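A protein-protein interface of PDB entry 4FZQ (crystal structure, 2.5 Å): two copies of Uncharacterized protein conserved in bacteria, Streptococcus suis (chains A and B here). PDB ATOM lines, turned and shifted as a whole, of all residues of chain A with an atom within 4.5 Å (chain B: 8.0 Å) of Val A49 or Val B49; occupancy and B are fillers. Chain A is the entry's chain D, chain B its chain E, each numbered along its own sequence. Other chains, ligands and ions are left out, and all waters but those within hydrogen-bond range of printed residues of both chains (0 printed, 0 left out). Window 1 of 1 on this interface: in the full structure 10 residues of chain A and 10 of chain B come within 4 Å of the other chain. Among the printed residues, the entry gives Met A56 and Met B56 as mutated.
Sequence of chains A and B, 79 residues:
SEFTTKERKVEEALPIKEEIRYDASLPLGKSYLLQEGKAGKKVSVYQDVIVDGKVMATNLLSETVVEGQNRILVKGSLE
The side-chain amide oxygen of Asn B59 is in hydrogen-bond range of the backbone NH of Phe A3, 3.0 Å away.
The side-chain carboxylate of Asp B52 lies within hydrogen-bond range of the side-chain hydroxyl of Ser B1.
The backbone NH of Val A49 sits at hydrogen-bond distance from the backbone carbonyl oxygen of Ala A57 (3.0 Å).
N of Met A56 is in hydrogen-bond range of O of Val A49, 2.9 Å away.
OG1 of Thr B58 sits close to OD1 of Asp B48, at 3.4 Å.
The backbone NH of Gln B47 lies within hydrogen-bond range of the backbone carbonyl oxygen of Asn B59 (3.0 Å).
The backbone NH of Val B49 is in hydrogen-bond range of the backbone carbonyl oxygen of Ala B57, 2.9 Å away.
Among the printed residues, pairs that only touch across the chains: Phe A3 with Gln B47 (3.4 Å), Phe A3 with Val B49 (3.1 Å), Phe A3 with Ala B57 (3.8 Å), Phe A3 with Thr B58 (3.996 Å), Gln A47 with Phe B3 (3.4 Å), Val A49 with Val B49 (3.8 Å), Val A51 with Ala B57 (3.7 Å), Met A56 with Met B56 (3.4 Å), Ala A57 with Ser B1 (3.1 Å), Ala A57 with Glu B2 (3.9 Å), Ala A57 with Phe B3 (3.9 Å) and Ala A57 with Val B51 (3.7 Å).
Thr A4 touches none of the printed residues of chain B.
Printed residues of chain B within 4 Å of Gln A47: Phe B3 (3.4 Å).
Val A49 touches one residue of chain B.
Of the printed residues of chain B, Val A51 touches Ala B57.
Lys A54 touches none of the printed residues of chain B.
Of the printed residues of chain A, Ser B1 touches Ala A57 (3.1 Å).
Of the printed residues of chain A, Gln B47 touches Phe A3 (3.4 Å).
Val B49 touches just these residues of chain A: Phe A3 (3.1 Å) and Val A49 (3.8 Å).
Of the printed residues of chain A, Asn B59 touches Phe A3.
The nearest residue of chain B that does not touch Val A49 is Phe B3 (4.04 Å).
Of the 21 printed residues of chain B, 10 touch a printed residue of chain A.
Printed residues of chain B that touch a printed residue of chain A: Ser B1, Glu B2, Phe B3, Gln B47, Val B49, Val B51, Met B56, Ala B57, Thr B58 and Asn B59.
Hydrophobic or aromatic side chains of chain B within 4 Å of the printed part of chain A: Phe B3, Val B49, Val B51, Met B56 and Ala B57.
Of the 11 printed residues of chain A, 6 touch a printed residue of chain B.
Printed residues of chain A that touch a printed residue of chain B: Phe A3, Gln A47, Val A49, Val A51, Met A56 and Ala A57.
Among the printed residues, no Asp or Glu carboxylate lies within 4 Å of a Lys or Arg side-chain nitrogen of the other chain.
Phe A3 touches Gln B47, and with the chains exchanged Gln A47 touches Phe B3.
Phe A3 touches Val B49, but with the chains exchanged Val A49 does not touch Phe B3 (4.04 Å).
Val A49 touches its own counterpart, Val B49.
Met A56 touches its own counterpart, Met B56.
Positions printed for both chains: 3, 4, 47, 48, 49, 50, 51, 54, 55, 56 and 57.
Of the 13 pairs that touch across the chains among the printed residues, 8 have their exchanged pair printed and touching as well.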
ATOM      1  N   PHE A   3     -10.475  -8.457  19.971  1.00  0.00           N
ATOM      2  CA  PHE A   3     -10.240  -9.104  18.692  1.00  0.00           C
ATOM      3  C   PHE A   3      -9.581  -8.166  17.701  1.00  0.00           C
ATOM      4  O   PHE A   3      -9.717  -6.950  17.795  1.00  0.00           O
ATOM      5  CB  PHE A   3     -11.562  -9.594  18.109  1.00  0.00           C
ATOM      6  CG  PHE A   3     -12.497  -8.484  17.710  1.00  0.00           C
ATOM      7  CD1 PHE A   3     -12.485  -7.977  16.412  1.00  0.00           C
ATOM      8  CD2 PHE A   3     -13.391  -7.945  18.634  1.00  0.00           C
ATOM      9  CE1 PHE A   3     -13.348  -6.942  16.042  1.00  0.00           C
ATOM     10  CE2 PHE A   3     -14.252  -6.914  18.274  1.00  0.00           C
ATOM     11  CZ  PHE A   3     -14.236  -6.411  16.973  1.00  0.00           C
ATOM     12  N   THR A   4      -8.849  -8.739  16.757  1.00  0.00           N
ATOM     13  CA  THR A   4      -8.204  -7.957  15.719  1.00  0.00           C
ATOM     14  C   THR A   4      -8.619  -8.623  14.424  1.00  0.00           C
ATOM     15  O   THR A   4      -9.234  -9.690  14.443  1.00  0.00           O
ATOM     16  CB  THR A   4      -6.663  -7.979  15.837  1.00  0.00           C
ATOM     17  OG1 THR A   4      -6.215  -9.336  15.917  1.00  0.00           O
ATOM     18  CG2 THR A   4      -6.200  -7.203  17.074  1.00  0.00           C
ATOM     19  N   GLN A  47     -10.925 -11.799   5.194  1.00  0.00           N
ATOM     20  CA  GLN A  47     -10.656 -11.008   6.369  1.00  0.00           C
ATOM     21  C   GLN A  47     -10.944 -11.932   7.545  1.00  0.00           C
ATOM     22  O   GLN A  47     -12.080 -12.399   7.715  1.00  0.00           O
ATOM     23  CB  GLN A  47     -11.554  -9.784   6.419  1.00  0.00           C
ATOM     24  CG  GLN A  47     -11.282  -8.916   7.626  1.00  0.00           C
ATOM     25  CD  GLN A  47     -12.099  -7.651   7.632  1.00  0.00           C
ATOM     26  OE1 GLN A  47     -13.313  -7.678   7.399  1.00  0.00           O
ATOM     27  NE2 GLN A  47     -11.442  -6.529   7.907  1.00  0.00           N
ATOM     28  N   ASP A  48      -9.908 -12.234   8.325  1.00  0.00           N
ATOM     29  CA  ASP A  48     -10.064 -13.108   9.485  1.00  0.00           C
ATOM     30  C   ASP A  48     -10.231 -12.324  10.786  1.00  0.00           C
ATOM     31  O   ASP A  48      -9.558 -11.316  11.004  1.00  0.00           O
ATOM     32  CB  ASP A  48      -8.847 -14.032   9.659  1.00  0.00           C
ATOM     33  CG  ASP A  48      -8.687 -15.043   8.528  1.00  0.00           C
ATOM     34  OD1 ASP A  48      -9.703 -15.606   8.039  1.00  0.00           O
ATOM     35  OD2 ASP A  48      -7.524 -15.295   8.148  1.00  0.00           O
ATOM     36  N   VAL A  49     -11.142 -12.776  11.643  1.00  0.00           N
ATOM     37  CA  VAL A  49     -11.307 -12.142  12.944  1.00  0.00           C
ATOM     38  C   VAL A  49     -10.486 -13.019  13.887  1.00  0.00           C
ATOM     39  O   VAL A  49     -10.764 -14.209  14.031  1.00  0.00           O
ATOM     40  CB  VAL A  49     -12.776 -12.110  13.412  1.00  0.00           C
ATOM     41  CG1 VAL A  49     -13.396 -13.489  13.313  1.00  0.00           C
ATOM     42  CG2 VAL A  49     -12.843 -11.616  14.853  1.00  0.00           C
ATOM     43  N   ILE A  50      -9.462 -12.426  14.497  1.00  0.00           N
ATOM     44  CA  ILE A  50      -8.559 -13.125  15.410  1.00  0.00           C
ATOM     45  C   ILE A  50      -8.881 -12.889  16.890  1.00  0.00           C
ATOM     46  O   ILE A  50      -8.908 -11.746  17.348  1.00  0.00           O
ATOM     47  CB  ILE A  50      -7.099 -12.657  15.218  1.00  0.00           C
ATOM     48  CG1 ILE A  50      -6.677 -12.767  13.752  1.00  0.00           C
ATOM     49  CG2 ILE A  50      -6.179 -13.470  16.122  1.00  0.00           C
ATOM     50  CD1 ILE A  50      -7.182 -11.646  12.857  1.00  0.00           C
ATOM     51  N   VAL A  51      -9.090 -13.970  17.637  1.00  0.00           N
ATOM     52  CA  VAL A  51      -9.364 -13.874  19.070  1.00  0.00           C
ATOM     53  C   VAL A  51      -8.440 -14.817  19.829  1.00  0.00           C
ATOM     54  O   VAL A  51      -8.418 -16.024  19.571  1.00  0.00           O
ATOM     55  CB  VAL A  51     -10.818 -14.233  19.406  1.00  0.00           C
ATOM     56  CG1 VAL A  51     -11.026 -14.203  20.909  1.00  0.00           C
ATOM     57  CG2 VAL A  51     -11.752 -13.243  18.741  1.00  0.00           C
ATOM     58  N   LYS A  54      -6.323 -17.055  17.837  1.00  0.00           N
ATOM     59  CA  LYS A  54      -6.997 -17.978  16.932  1.00  0.00           C
ATOM     60  C   LYS A  54      -8.028 -17.320  15.995  1.00  0.00           C
ATOM     61  O   LYS A  54      -8.798 -16.444  16.412  1.00  0.00           O
ATOM     62  CB  LYS A  54      -7.673 -19.079  17.755  1.00  0.00           C
ATOM     63  CG  LYS A  54      -8.365 -20.159  16.939  1.00  0.00           C
ATOM     64  CD  LYS A  54      -9.074 -21.163  17.842  1.00  0.00           C
ATOM     65  CE  LYS A  54      -8.092 -21.840  18.803  1.00  0.00           C
ATOM     66  NZ  LYS A  54      -8.755 -22.802  19.739  1.00  0.00           N
ATOM     67  N   VAL A  55      -8.030 -17.737  14.726  1.00  0.00           N
ATOM     68  CA  VAL A  55      -8.995 -17.228  13.751  1.00  0.00           C
ATOM     69  C   VAL A  55     -10.346 -17.857  14.103  1.00  0.00           C
ATOM     70  O   VAL A  55     -10.507 -19.072  14.028  1.00  0.00           O
ATOM     71  CB  VAL A  55      -8.613 -17.629  12.303  1.00  0.00           C
ATOM     72  CG1 VAL A  55      -9.768 -17.327  11.349  1.00  0.00           C
ATOM     73  CG2 VAL A  55      -7.373 -16.880  11.870  1.00  0.00           C
ATOM     74  N   MET A  56     -11.311 -17.032  14.491  1.00  0.00           N
ATOM     75  CA  MET A  56     -12.621 -17.533  14.882  1.00  0.00           C
ATOM     76  C   MET A  56     -13.657 -17.409  13.787  1.00  0.00           C
ATOM     77  O   MET A  56     -14.773 -17.894  13.932  1.00  0.00           O
ATOM     78  CB  MET A  56     -13.130 -16.793  16.124  1.00  0.00           C
ATOM     79  CG  MET A  56     -12.270 -16.978  17.365  1.00  0.00           C
ATOM     80  SD  MET A  56     -11.849 -18.707  17.655  1.00  0.00           S
ATOM     81  CE  MET A  56     -13.443 -19.346  18.172  1.00  0.00           C
ATOM     82  N   ALA A  57     -13.292 -16.750  12.695  1.00  0.00           N
ATOM     83  CA  ALA A  57     -14.219 -16.558  11.589  1.00  0.00           C
ATOM     84  C   ALA A  57     -13.538 -15.801  10.461  1.00  0.00           C
ATOM     85  O   ALA A  57     -12.442 -15.264  10.624  1.00  0.00           O
ATOM     86  CB  ALA A  57     -15.449 -15.798  12.068  1.00  0.00           C
ATOM     87  N   SER B   1     -17.066 -19.836   9.799  1.00  0.00           N
ATOM     88  CA  SER B   1     -18.287 -19.052   9.472  1.00  0.00           C
ATOM     89  C   SER B   1     -17.940 -17.590   9.274  1.00  0.00           C
ATOM     90  O   SER B   1     -16.856 -17.138   9.637  1.00  0.00           O
ATOM     91  CB  SER B   1     -19.300 -19.156  10.608  1.00  0.00           C
ATOM     92  OG  SER B   1     -19.311 -20.463  11.152  1.00  0.00           O
ATOM     93  N   GLU B   2     -18.872 -16.853   8.690  1.00  0.00           N
ATOM     94  CA  GLU B   2     -18.683 -15.434   8.473  1.00  0.00           C
ATOM     95  C   GLU B   2     -18.874 -14.755   9.817  1.00  0.00           C
ATOM     96  O   GLU B   2     -19.163 -15.408  10.818  1.00  0.00           O
ATOM     97  CB  GLU B   2     -19.715 -14.903   7.477  1.00  0.00           C
ATOM     98  CG  GLU B   2     -19.352 -15.138   6.021  1.00  0.00           C
ATOM     99  CD  GLU B   2     -20.477 -14.772   5.070  1.00  0.00           C
ATOM    100  OE1 GLU B   2     -21.133 -13.732   5.293  1.00  0.00           O
ATOM    101  OE2 GLU B   2     -20.702 -15.520   4.093  1.00  0.00           O
ATOM    102  N   PHE B   3     -18.686 -13.448   9.848  1.00  0.00           N
ATOM    103  CA  PHE B   3     -18.885 -12.720  11.084  1.00  0.00           C
ATOM    104  C   PHE B   3     -19.485 -11.368  10.774  1.00  0.00           C
ATOM    105  O   PHE B   3     -19.500 -10.926   9.625  1.00  0.00           O
ATOM    106  CB  PHE B   3     -17.574 -12.548  11.867  1.00  0.00           C
ATOM    107  CG  PHE B   3     -16.558 -11.658  11.196  1.00  0.00           C
ATOM    108  CD1 PHE B   3     -15.676 -12.171  10.247  1.00  0.00           C
ATOM    109  CD2 PHE B   3     -16.472 -10.312  11.529  1.00  0.00           C
ATOM    110  CE1 PHE B   3     -14.723 -11.356   9.639  1.00  0.00           C
ATOM    111  CE2 PHE B   3     -15.521  -9.488  10.927  1.00  0.00           C
ATOM    112  CZ  PHE B   3     -14.643 -10.016   9.978  1.00  0.00           C
ATOM    113  N   THR B   4     -19.999 -10.725  11.808  1.00  0.00           N
ATOM    114  CA  THR B   4     -20.604  -9.418  11.667  1.00  0.00           C
ATOM    115  C   THR B   4     -20.278  -8.655  12.924  1.00  0.00           C
ATOM    116  O   THR B   4     -19.902  -9.245  13.926  1.00  0.00           O
ATOM    117  CB  THR B   4     -22.124  -9.528  11.508  1.00  0.00           C
ATOM    118  OG1 THR B   4     -22.733  -8.308  11.952  1.00  0.00           O
ATOM    119  CG2 THR B   4     -22.667 -10.700  12.318  1.00  0.00           C
ATOM    120  N   THR B   5     -20.398  -7.342  12.879  1.00  0.00           N
ATOM    121  CA  THR B   5     -20.101  -6.553  14.061  1.00  0.00           C
ATOM    122  C   THR B   5     -21.329  -5.784  14.510  1.00  0.00           C
ATOM    123  O   THR B   5     -22.308  -5.667  13.774  1.00  0.00           O
ATOM    124  CB  THR B   5     -18.952  -5.571  13.806  1.00  0.00           C
ATOM    125  OG1 THR B   5     -19.240  -4.806  12.629  1.00  0.00           O
ATOM    126  CG2 THR B   5     -17.641  -6.327  13.640  1.00  0.00           C
ATOM    127  N   LYS B   6     -21.269  -5.260  15.725  1.00  0.00           N
ATOM    128  CA  LYS B   6     -22.375  -4.506  16.280  1.00  0.00           C
ATOM    129  C   LYS B   6     -21.831  -3.644  17.408  1.00  0.00           C
ATOM    130  O   LYS B   6     -20.981  -4.088  18.179  1.00  0.00           O
ATOM    131  CB  LYS B   6     -23.439  -5.470  16.809  1.00  0.00           C
ATOM    132  CG  LYS B   6     -24.591  -4.804  17.537  1.00  0.00           C
ATOM    133  CD  LYS B   6     -25.187  -5.756  18.572  1.00  0.00           C
ATOM    134  CE  LYS B   6     -24.206  -6.016  19.713  1.00  0.00           C
ATOM    135  NZ  LYS B   6     -24.629  -7.150  20.582  1.00  0.00           N
ATOM    136  N   GLU B   7     -22.326  -2.415  17.495  1.00  0.00           N
ATOM    137  CA  GLU B   7     -21.893  -1.483  18.525  1.00  0.00           C
ATOM    138  C   GLU B   7     -22.860  -1.388  19.700  1.00  0.00           C
ATOM    139  O   GLU B   7     -24.067  -1.236  19.519  1.00  0.00           O
ATOM    140  CB  GLU B   7     -21.695  -0.096  17.920  1.00  0.00           C
ATOM    141  CG  GLU B   7     -20.484  -0.007  17.023  1.00  0.00           C
ATOM    142  CD  GLU B   7     -20.348   1.343  16.348  1.00  0.00           C
ATOM    143  OE1 GLU B   7     -20.504   2.377  17.036  1.00  0.00           O
ATOM    144  OE2 GLU B   7     -20.072   1.363  15.129  1.00  0.00           O
ATOM    145  N   TYR B  46     -18.818  -0.036  22.762  1.00  0.00           N
ATOM    146  CA  TYR B  46     -18.143  -1.277  22.386  1.00  0.00           C
ATOM    147  C   TYR B  46     -18.581  -1.748  21.018  1.00  0.00           C
ATOM    148  O   TYR B  46     -19.607  -1.319  20.494  1.00  0.00           O
ATOM    149  CB  TYR B  46     -18.460  -2.411  23.368  1.00  0.00           C
ATOM    150  CG  TYR B  46     -18.076  -2.148  24.797  1.00  0.00           C
ATOM    151  CD1 TYR B  46     -18.997  -1.619  25.698  1.00  0.00           C
ATOM    152  CD2 TYR B  46     -16.788  -2.420  25.250  1.00  0.00           C
ATOM    153  CE1 TYR B  46     -18.646  -1.372  27.021  1.00  0.00           C
ATOM    154  CE2 TYR B  46     -16.422  -2.169  26.567  1.00  0.00           C
ATOM    155  CZ  TYR B  46     -17.352  -1.648  27.445  1.00  0.00           C
ATOM    156  OH  TYR B  46     -16.989  -1.399  28.746  1.00  0.00           O
ATOM    157  N   GLN B  47     -17.791  -2.644  20.443  1.00  0.00           N
ATOM    158  CA  GLN B  47     -18.116  -3.235  19.153  1.00  0.00           C
ATOM    159  C   GLN B  47     -17.903  -4.728  19.337  1.00  0.00           C
ATOM    160  O   GLN B  47     -16.786  -5.171  19.630  1.00  0.00           O
ATOM    161  CB  GLN B  47     -17.206  -2.703  18.050  1.00  0.00           C
ATOM    162  CG  GLN B  47     -17.567  -3.267  16.695  1.00  0.00           C
ATOM    163  CD  GLN B  47     -16.611  -2.844  15.613  1.00  0.00           C
ATOM    164  OE1 GLN B  47     -15.396  -2.914  15.786  1.00  0.00           O
ATOM    165  NE2 GLN B  47     -17.154  -2.417  14.474  1.00  0.00           N
ATOM    166  N   ASP B  48     -18.976  -5.499  19.191  1.00  0.00           N
ATOM    167  CA  ASP B  48     -18.891  -6.940  19.371  1.00  0.00           C
ATOM    168  C   ASP B  48     -18.789  -7.671  18.043  1.00  0.00           C
ATOM    169  O   ASP B  48     -19.357  -7.237  17.050  1.00  0.00           O
ATOM    170  CB  ASP B  48     -20.129  -7.468  20.108  1.00  0.00           C
ATOM    171  CG  ASP B  48     -20.386  -6.761  21.431  1.00  0.00           C
ATOM    172  OD1 ASP B  48     -19.460  -6.682  22.270  1.00  0.00           O
ATOM    173  OD2 ASP B  48     -21.527  -6.295  21.634  1.00  0.00           O
ATOM    174  N   VAL B  49     -18.055  -8.775  18.025  1.00  0.00           N
ATOM    175  CA  VAL B  49     -17.959  -9.581  16.821  1.00  0.00           C
ATOM    176  C   VAL B  49     -18.966 -10.702  17.029  1.00  0.00           C
ATOM    177  O   VAL B  49     -18.937 -11.388  18.055  1.00  0.00           O
ATOM    178  CB  VAL B  49     -16.572 -10.234  16.640  1.00  0.00           C
ATOM    179  CG1 VAL B  49     -16.581 -11.152  15.415  1.00  0.00           C
ATOM    180  CG2 VAL B  49     -15.535  -9.182  16.464  1.00  0.00           C
ATOM    181  N   ILE B  50     -19.856 -10.882  16.062  1.00  0.00           N
ATOM    182  CA  ILE B  50     -20.850 -11.928  16.165  1.00  0.00           C
ATOM    183  C   ILE B  50     -20.605 -13.048  15.165  1.00  0.00           C
ATOM    184  O   ILE B  50     -20.427 -12.815  13.971  1.00  0.00           O
ATOM    185  CB  ILE B  50     -22.284 -11.372  15.975  1.00  0.00           C
ATOM    186  CG1 ILE B  50     -22.714 -10.564  17.206  1.00  0.00           C
ATOM    187  CG2 ILE B  50     -23.258 -12.516  15.790  1.00  0.00           C
ATOM    188  CD1 ILE B  50     -22.957 -11.350  18.499  1.00  0.00           C
ATOM    189  N   VAL B  51     -20.586 -14.267  15.685  1.00  0.00           N
ATOM    190  CA  VAL B  51     -20.387 -15.468  14.893  1.00  0.00           C
ATOM    191  C   VAL B  51     -21.461 -16.463  15.311  1.00  0.00           C
ATOM    192  O   VAL B  51     -21.599 -16.780  16.498  1.00  0.00           O
ATOM    193  CB  VAL B  51     -19.015 -16.090  15.159  1.00  0.00           C
ATOM    194  CG1 VAL B  51     -18.916 -17.442  14.475  1.00  0.00           C
ATOM    195  CG2 VAL B  51     -17.931 -15.164  14.669  1.00  0.00           C
ATOM    196  N   ASP B  52     -22.222 -16.950  14.336  1.00  0.00           N
ATOM    197  CA  ASP B  52     -23.299 -17.903  14.606  1.00  0.00           C
ATOM    198  C   ASP B  52     -24.223 -17.373  15.711  1.00  0.00           C
ATOM    199  O   ASP B  52     -24.575 -18.098  16.642  1.00  0.00           O
ATOM    200  CB  ASP B  52     -22.719 -19.265  15.022  1.00  0.00           C
ATOM    201  CG  ASP B  52     -21.831 -19.883  13.947  1.00  0.00           C
ATOM    202  OD1 ASP B  52     -22.150 -19.724  12.743  1.00  0.00           O
ATOM    203  OD2 ASP B  52     -20.826 -20.550  14.303  1.00  0.00           O
ATOM    204  N   GLY B  53     -24.604 -16.102  15.608  1.00  0.00           N
ATOM    205  CA  GLY B  53     -25.482 -15.506  16.599  1.00  0.00           C
ATOM    206  C   GLY B  53     -24.960 -15.491  18.030  1.00  0.00           C
ATOM    207  O   GLY B  53     -25.729 -15.665  18.970  1.00  0.00           O
ATOM    208  N   LYS B  54     -23.660 -15.272  18.201  1.00  0.00           N
ATOM    209  CA  LYS B  54     -23.054 -15.228  19.530  1.00  0.00           C
ATOM    210  C   LYS B  54     -21.911 -14.224  19.586  1.00  0.00           C
ATOM    211  O   LYS B  54     -21.027 -14.236  18.724  1.00  0.00           O
ATOM    212  CB  LYS B  54     -22.490 -16.597  19.910  1.00  0.00           C
ATOM    213  CG  LYS B  54     -23.508 -17.627  20.362  1.00  0.00           C
ATOM    214  CD  LYS B  54     -23.316 -18.938  19.602  1.00  0.00           C
ATOM    215  CE  LYS B  54     -21.882 -19.456  19.694  1.00  0.00           C
ATOM    216  NZ  LYS B  54     -21.649 -20.615  18.778  1.00  0.00           N
ATOM    217  N   VAL B  55     -21.920 -13.361  20.596  1.00  0.00           N
ATOM    218  CA  VAL B  55     -20.834 -12.407  20.736  1.00  0.00           C
ATOM    219  C   VAL B  55     -19.604 -13.232  21.107  1.00  0.00           C
ATOM    220  O   VAL B  55     -19.607 -13.922  22.125  1.00  0.00           O
ATOM    221  CB  VAL B  55     -21.127 -11.364  21.829  1.00  0.00           C
ATOM    222  CG1 VAL B  55     -19.952 -10.411  21.973  1.00  0.00           C
ATOM    223  CG2 VAL B  55     -22.377 -10.582  21.470  1.00  0.00           C
ATOM    224  N   MET B  56     -18.570 -13.172  20.267  1.00  0.00           N
ATOM    225  CA  MET B  56     -17.342 -13.935  20.483  1.00  0.00           C
ATOM    226  C   MET B  56     -16.222 -13.106  21.099  1.00  0.00           C
ATOM    227  O   MET B  56     -15.276 -13.651  21.674  1.00  0.00           O
ATOM    228  CB  MET B  56     -16.851 -14.513  19.155  1.00  0.00           C
ATOM    229  CG  MET B  56     -17.822 -15.488  18.488  1.00  0.00           C
ATOM    230  SD  MET B  56     -17.940 -17.087  19.332  1.00  0.00           S
ATOM    231  CE  MET B  56     -16.351 -17.790  18.861  1.00  0.00           C
ATOM    232  N   ALA B  57     -16.326 -11.789  20.967  1.00  0.00           N
ATOM    233  CA  ALA B  57     -15.312 -10.893  21.498  1.00  0.00           C
ATOM    234  C   ALA B  57     -15.803  -9.465  21.362  1.00  0.00           C
ATOM    235  O   ALA B  57     -16.694  -9.174  20.561  1.00  0.00           O
ATOM    236  CB  ALA B  57     -13.999 -11.067  20.738  1.00  0.00           C
ATOM    237  N   THR B  58     -15.213  -8.565  22.136  1.00  0.00           N
ATOM    238  CA  THR B  58     -15.628  -7.177  22.086  1.00  0.00           C
ATOM    239  C   THR B  58     -14.471  -6.225  22.339  1.00  0.00           C
ATOM    240  O   THR B  58     -13.560  -6.526  23.112  1.00  0.00           O
ATOM    241  CB  THR B  58     -16.767  -6.910  23.108  1.00  0.00           C
ATOM    242  OG1 THR B  58     -16.535  -5.662  23.769  1.00  0.00           O
ATOM    243  CG2 THR B  58     -16.846  -8.030  24.127  1.00  0.00           C
ATOM    244  N   ASN B  59     -14.505  -5.083  21.662  1.00  0.00           N
ATOM    245  CA  ASN B  59     -13.467  -4.072  21.815  1.00  0.00           C
ATOM    246  C   ASN B  59     -14.101  -2.783  22.284  1.00  0.00           C
ATOM    247  O   ASN B  59     -15.260  -2.496  21.965  1.00  0.00           O
ATOM    248  CB  ASN B  59     -12.761  -3.775  20.487  1.00  0.00           C
ATOM    249  CG  ASN B  59     -12.000  -4.955  19.944  1.00  0.00           C
ATOM    250  OD1 ASN B  59     -11.507  -5.789  20.695  1.00  0.00           O
ATOM    251  ND2 ASN B  59     -11.877  -5.017  18.623  1.00  0.00           N
